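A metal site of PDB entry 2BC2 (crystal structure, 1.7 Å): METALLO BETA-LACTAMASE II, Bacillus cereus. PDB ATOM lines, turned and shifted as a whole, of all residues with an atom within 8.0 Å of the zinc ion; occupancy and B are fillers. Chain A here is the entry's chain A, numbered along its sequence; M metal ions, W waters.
The zinc ion is bound by a ring nitrogen (ND1) of His 88 (2.0 Å), a ring nitrogen (NE2) of His 149 (2.1 Å), water W1 (2.1 Å) and a ring nitrogen (NE2) of His 86 (2.3 Å).
Slightly farther from the zinc ion lies water W2 (2.7 Å).
A ring nitrogen (NE2) of His 88 sits at hydrogen-bond distance from the side-chain carboxylate (OD2) of Asp 183 (3.1 Å).
N of His 149 sits at hydrogen-bond distance from OD1 of Asn 153, at 2.8 Å.
The side-chain carboxylate (OD2) of Asp 90 lies close to OD1 of CSD 168, 3.0 Å away.
The guanidinium group of Arg 91 lies within salt-bridge range of OD2 of CSD 168, 3.2 Å away.
The side-chain amino group of Lys 171 sits at hydrogen-bond distance from O of CSD 168 (3.1 Å).
Water W1 lies within hydrogen-bond range of the side-chain carboxylate (OD1) of Asp 90 (2.7 Å) and OD1 of CSD 168 (3.0 Å).
OD1 of CSD 168 touches the zinc ion, 3.7 Å away.
Within 4 Å of the zinc ion: His 86, His 88, His 149 and CSD 168.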
ATOM      1  N   TRP A  59      21.103 -11.426  32.956  1.00  0.00           N
ATOM      2  CA  TRP A  59      19.856 -11.895  32.335  1.00  0.00           C
ATOM      3  C   TRP A  59      19.124 -10.914  31.444  1.00  0.00           C
ATOM      4  O   TRP A  59      18.658 -11.283  30.367  1.00  0.00           O
ATOM      5  CB  TRP A  59      18.909 -12.430  33.413  1.00  0.00           C
ATOM      6  CG  TRP A  59      19.478 -13.575  34.205  1.00  0.00           C
ATOM      7  CD1 TRP A  59      20.096 -13.507  35.425  1.00  0.00           C
ATOM      8  CD2 TRP A  59      19.505 -14.961  33.831  1.00  0.00           C
ATOM      9  NE1 TRP A  59      20.500 -14.761  35.825  1.00  0.00           N
ATOM     10  CE2 TRP A  59      20.145 -15.672  34.873  1.00  0.00           C
ATOM     11  CE3 TRP A  59      19.043 -15.670  32.710  1.00  0.00           C
ATOM     12  CZ2 TRP A  59      20.335 -17.060  34.821  1.00  0.00           C
ATOM     13  CZ3 TRP A  59      19.235 -17.062  32.666  1.00  0.00           C
ATOM     14  CH2 TRP A  59      19.874 -17.733  33.719  1.00  0.00           C
ATOM     15  N   THR A  85      30.753 -14.282  26.965  1.00  0.00           N
ATOM     16  CA  THR A  85      31.182 -15.664  26.692  1.00  0.00           C
ATOM     17  C   THR A  85      30.355 -16.498  25.696  1.00  0.00           C
ATOM     18  O   THR A  85      30.846 -17.484  25.149  1.00  0.00           O
ATOM     19  CB  THR A  85      31.481 -16.449  27.975  1.00  0.00           C
ATOM     20  OG1 THR A  85      30.306 -16.532  28.777  1.00  0.00           O
ATOM     21  CG2 THR A  85      32.593 -15.754  28.767  1.00  0.00           C
ATOM     22  N   HIS A  86      29.093 -16.139  25.519  1.00  0.00           N
ATOM     23  CA  HIS A  86      28.220 -16.784  24.530  1.00  0.00           C
ATOM     24  C   HIS A  86      26.930 -15.979  24.366  1.00  0.00           C
ATOM     25  O   HIS A  86      26.637 -15.106  25.191  1.00  0.00           O
ATOM     26  CB  HIS A  86      28.010 -18.301  24.758  1.00  0.00           C
ATOM     27  CG  HIS A  86      27.083 -18.652  25.873  1.00  0.00           C
ATOM     28  ND1 HIS A  86      27.487 -18.741  27.192  1.00  0.00           N
ATOM     29  CD2 HIS A  86      25.770 -18.985  25.868  1.00  0.00           C
ATOM     30  CE1 HIS A  86      26.473 -19.123  27.939  1.00  0.00           C
ATOM     31  NE2 HIS A  86      25.417 -19.283  27.166  1.00  0.00           N
ATOM     32  N   ALA A  87      26.225 -16.215  23.271  1.00  0.00           N
ATOM     33  CA  ALA A  87      25.007 -15.466  22.958  1.00  0.00           C
ATOM     34  C   ALA A  87      23.671 -15.850  23.599  1.00  0.00           C
ATOM     35  O   ALA A  87      22.638 -15.850  22.929  1.00  0.00           O
ATOM     36  CB  ALA A  87      24.853 -15.349  21.440  1.00  0.00           C
ATOM     37  N   HIS A  88      23.675 -16.157  24.898  1.00  0.00           N
ATOM     38  CA  HIS A  88      22.437 -16.477  25.611  1.00  0.00           C
ATOM     39  C   HIS A  88      22.120 -15.369  26.612  1.00  0.00           C
ATOM     40  O   HIS A  88      23.006 -14.628  27.039  1.00  0.00           O
ATOM     41  CB  HIS A  88      22.524 -17.849  26.314  1.00  0.00           C
ATOM     42  CG  HIS A  88      22.309 -19.014  25.394  1.00  0.00           C
ATOM     43  ND1 HIS A  88      22.629 -20.314  25.752  1.00  0.00           N
ATOM     44  CD2 HIS A  88      21.798 -19.084  24.139  1.00  0.00           C
ATOM     45  CE1 HIS A  88      22.319 -21.121  24.755  1.00  0.00           C
ATOM     46  NE2 HIS A  88      21.819 -20.404  23.766  1.00  0.00           N
ATOM     47  N   ALA A  89      20.840 -15.273  26.990  1.00  0.00           N
ATOM     48  CA  ALA A  89      20.354 -14.244  27.905  1.00  0.00           C
ATOM     49  C   ALA A  89      21.219 -13.967  29.137  1.00  0.00           C
ATOM     50  O   ALA A  89      21.525 -12.805  29.426  1.00  0.00           O
ATOM     51  CB  ALA A  89      18.927 -14.553  28.340  1.00  0.00           C
ATOM     52  N   ASP A  90      21.614 -15.016  29.855  1.00  0.00           N
ATOM     53  CA  ASP A  90      22.421 -14.833  31.051  1.00  0.00           C
ATOM     54  C   ASP A  90      23.787 -14.195  30.804  1.00  0.00           C
ATOM     55  O   ASP A  90      24.404 -13.650  31.724  1.00  0.00           O
ATOM     56  CB  ASP A  90      22.594 -16.163  31.804  1.00  0.00           C
ATOM     57  CG  ASP A  90      23.343 -17.221  30.992  1.00  0.00           C
ATOM     58  OD1 ASP A  90      23.310 -17.179  29.742  1.00  0.00           O
ATOM     59  OD2 ASP A  90      23.964 -18.109  31.622  1.00  0.00           O
ATOM     60  N   ARG A  91      24.239 -14.227  29.551  1.00  0.00           N
ATOM     61  CA  ARG A  91      25.545 -13.680  29.198  1.00  0.00           C
ATOM     62  C   ARG A  91      25.468 -12.333  28.479  1.00  0.00           C
ATOM     63  O   ARG A  91      26.208 -11.404  28.806  1.00  0.00           O
ATOM     64  CB  ARG A  91      26.304 -14.658  28.300  1.00  0.00           C
ATOM     65  CG  ARG A  91      26.399 -16.060  28.847  1.00  0.00           C
ATOM     66  CD  ARG A  91      27.170 -16.081  30.148  1.00  0.00           C
ATOM     67  NE  ARG A  91      26.631 -17.066  31.097  1.00  0.00           N
ATOM     68  CZ  ARG A  91      27.132 -17.291  32.312  1.00  0.00           C
ATOM     69  NH1 ARG A  91      28.187 -16.608  32.742  1.00  0.00           N
ATOM     70  NH2 ARG A  91      26.538 -18.155  33.118  1.00  0.00           N
ATOM     71  N   HIS A 149      28.639 -26.086  25.104  1.00  0.00           N
ATOM     72  CA  HIS A 149      27.333 -25.636  25.584  1.00  0.00           C
ATOM     73  C   HIS A 149      26.586 -24.958  24.431  1.00  0.00           C
ATOM     74  O   HIS A 149      25.364 -25.064  24.298  1.00  0.00           O
ATOM     75  CB  HIS A 149      27.510 -24.652  26.738  1.00  0.00           C
ATOM     76  CG  HIS A 149      26.254 -23.934  27.119  1.00  0.00           C
ATOM     77  ND1 HIS A 149      25.142 -24.585  27.606  1.00  0.00           N
ATOM     78  CD2 HIS A 149      25.919 -22.618  27.049  1.00  0.00           C
ATOM     79  CE1 HIS A 149      24.181 -23.710  27.824  1.00  0.00           C
ATOM     80  NE2 HIS A 149      24.628 -22.511  27.493  1.00  0.00           N
ATOM     81  N   THR A 150      27.354 -24.227  23.622  1.00  0.00           N
ATOM     82  CA  THR A 150      26.865 -23.547  22.427  1.00  0.00           C
ATOM     83  C   THR A 150      27.978 -23.655  21.387  1.00  0.00           C
ATOM     84  O   THR A 150      29.095 -24.102  21.686  1.00  0.00           O
ATOM     85  CB  THR A 150      26.541 -22.043  22.662  1.00  0.00           C
ATOM     86  OG1 THR A 150      27.690 -21.358  23.176  1.00  0.00           O
ATOM     87  CG2 THR A 150      25.380 -21.883  23.625  1.00  0.00           C
ATOM     88  N   ASP A 152      29.406 -21.168  19.990  1.00  0.00           N
ATOM     89  CA  ASP A 152      30.313 -20.032  20.208  1.00  0.00           C
ATOM     90  C   ASP A 152      31.000 -19.845  21.545  1.00  0.00           C
ATOM     91  O   ASP A 152      31.853 -18.954  21.667  1.00  0.00           O
ATOM     92  CB  ASP A 152      29.542 -18.741  19.882  1.00  0.00           C
ATOM     93  CG  ASP A 152      28.404 -18.476  20.861  1.00  0.00           C
ATOM     94  OD1 ASP A 152      27.643 -19.410  21.158  1.00  0.00           O
ATOM     95  OD2 ASP A 152      28.276 -17.331  21.348  1.00  0.00           O
ATOM     96  N   ASN A 153      30.666 -20.644  22.550  1.00  0.00           N
ATOM     97  CA  ASN A 153      31.263 -20.488  23.879  1.00  0.00           C
ATOM     98  C   ASN A 153      32.782 -20.350  23.978  1.00  0.00           C
ATOM     99  O   ASN A 153      33.541 -21.086  23.346  1.00  0.00           O
ATOM    100  CB  ASN A 153      30.748 -21.553  24.872  1.00  0.00           C
ATOM    101  CG  ASN A 153      31.011 -22.997  24.417  1.00  0.00           C
ATOM    102  OD1 ASN A 153      30.322 -23.916  24.856  1.00  0.00           O
ATOM    103  ND2 ASN A 153      31.988 -23.207  23.546  1.00  0.00           N
ATOM    104  N   GLY A 167      32.470 -20.304  32.156  1.00  0.00           N
ATOM    105  CA  GLY A 167      31.161 -19.999  31.591  1.00  0.00           C
ATOM    106  C   GLY A 167      30.294 -21.245  31.686  1.00  0.00           C
ATOM    107  O   GLY A 167      30.531 -22.133  32.524  1.00  0.00           O
ATOM    108  N   CSD A 168      29.316 -21.364  30.792  1.00  0.00           N
ATOM    109  CA  CSD A 168      28.431 -22.519  30.824  1.00  0.00           C
ATOM    110  CB  CSD A 168      27.079 -22.158  30.218  1.00  0.00           C
ATOM    111  SG  CSD A 168      26.269 -20.850  31.176  1.00  0.00           S
ATOM    112  C   CSD A 168      29.020 -23.791  30.219  1.00  0.00           C
ATOM    113  O   CSD A 168      28.329 -24.828  30.136  1.00  0.00           O
ATOM    114  OD1 CSD A 168      24.755 -20.913  30.896  1.00  0.00           O
ATOM    115  OD2 CSD A 168      26.417 -21.323  32.575  1.00  0.00           O
ATOM    116  N   LEU A 169      30.283 -23.732  29.824  1.00  0.00           N
ATOM    117  CA  LEU A 169      30.995 -24.892  29.288  1.00  0.00           C
ATOM    118  C   LEU A 169      31.374 -25.784  30.496  1.00  0.00           C
ATOM    119  O   LEU A 169      31.634 -26.978  30.359  1.00  0.00           O
ATOM    120  CB  LEU A 169      32.283 -24.447  28.574  1.00  0.00           C
ATOM    121  CG  LEU A 169      33.146 -25.518  27.892  1.00  0.00           C
ATOM    122  CD1 LEU A 169      32.575 -25.895  26.532  1.00  0.00           C
ATOM    123  CD2 LEU A 169      34.567 -25.012  27.724  1.00  0.00           C
ATOM    124  N   LYS A 171      30.282 -27.045  34.421  1.00  0.00           N
ATOM    125  CA  LYS A 171      29.237 -27.208  35.418  1.00  0.00           C
ATOM    126  C   LYS A 171      29.823 -27.222  36.832  1.00  0.00           C
ATOM    127  O   LYS A 171      30.978 -27.604  37.030  1.00  0.00           O
ATOM    128  CB  LYS A 171      28.485 -28.532  35.172  1.00  0.00           C
ATOM    129  CG  LYS A 171      27.927 -28.682  33.769  1.00  0.00           C
ATOM    130  CD  LYS A 171      26.949 -27.575  33.446  1.00  0.00           C
ATOM    131  CE  LYS A 171      26.928 -27.295  31.964  1.00  0.00           C
ATOM    132  NZ  LYS A 171      25.969 -26.226  31.605  1.00  0.00           N
ATOM    133  N   LEU A 178      23.337 -30.939  32.531  1.00  0.00           N
ATOM    134  CA  LEU A 178      24.110 -30.115  31.609  1.00  0.00           C
ATOM    135  C   LEU A 178      23.398 -28.820  31.215  1.00  0.00           C
ATOM    136  O   LEU A 178      24.004 -27.918  30.634  1.00  0.00           O
ATOM    137  CB  LEU A 178      24.444 -30.897  30.339  1.00  0.00           C
ATOM    138  CG  LEU A 178      25.373 -32.097  30.496  1.00  0.00           C
ATOM    139  CD1 LEU A 178      25.375 -32.913  29.221  1.00  0.00           C
ATOM    140  CD2 LEU A 178      26.778 -31.605  30.843  1.00  0.00           C
ATOM    141  N   GLY A 179      22.111 -28.732  31.544  1.00  0.00           N
ATOM    142  CA  GLY A 179      21.329 -27.554  31.218  1.00  0.00           C
ATOM    143  C   GLY A 179      20.708 -27.648  29.835  1.00  0.00           C
ATOM    144  O   GLY A 179      20.444 -28.746  29.341  1.00  0.00           O
ATOM    145  N   ASN A 180      20.482 -26.493  29.219  1.00  0.00           N
ATOM    146  CA  ASN A 180      19.891 -26.406  27.880  1.00  0.00           C
ATOM    147  C   ASN A 180      20.892 -26.936  26.846  1.00  0.00           C
ATOM    148  O   ASN A 180      21.979 -26.364  26.656  1.00  0.00           O
ATOM    149  CB  ASN A 180      19.536 -24.936  27.585  1.00  0.00           C
ATOM    150  CG  ASN A 180      18.871 -24.738  26.228  1.00  0.00           C
ATOM    151  OD1 ASN A 180      19.050 -25.536  25.305  1.00  0.00           O
ATOM    152  ND2 ASN A 180      18.102 -23.668  26.106  1.00  0.00           N
ATOM    153  N   ASP A 183      20.948 -25.949  21.829  1.00  0.00           N
ATOM    154  CA  ASP A 183      21.930 -25.236  21.011  1.00  0.00           C
ATOM    155  C   ASP A 183      23.322 -25.779  21.259  1.00  0.00           C
ATOM    156  O   ASP A 183      24.313 -25.215  20.786  1.00  0.00           O
ATOM    157  CB  ASP A 183      21.928 -23.738  21.348  1.00  0.00           C
ATOM    158  CG  ASP A 183      20.557 -23.100  21.157  1.00  0.00           C
ATOM    159  OD1 ASP A 183      19.889 -23.376  20.137  1.00  0.00           O
ATOM    160  OD2 ASP A 183      20.159 -22.306  22.044  1.00  0.00           O
HETATM  161 ZN    ZN M   1      23.652 -20.697  27.396  1.00  0.00          ZN
HETATM  162  O   HOH W   1      22.743 -19.765  29.039  1.00  0.00           O
HETATM  163  O   HOH W   2      21.428 -21.883  28.257  1.00  0.00           O
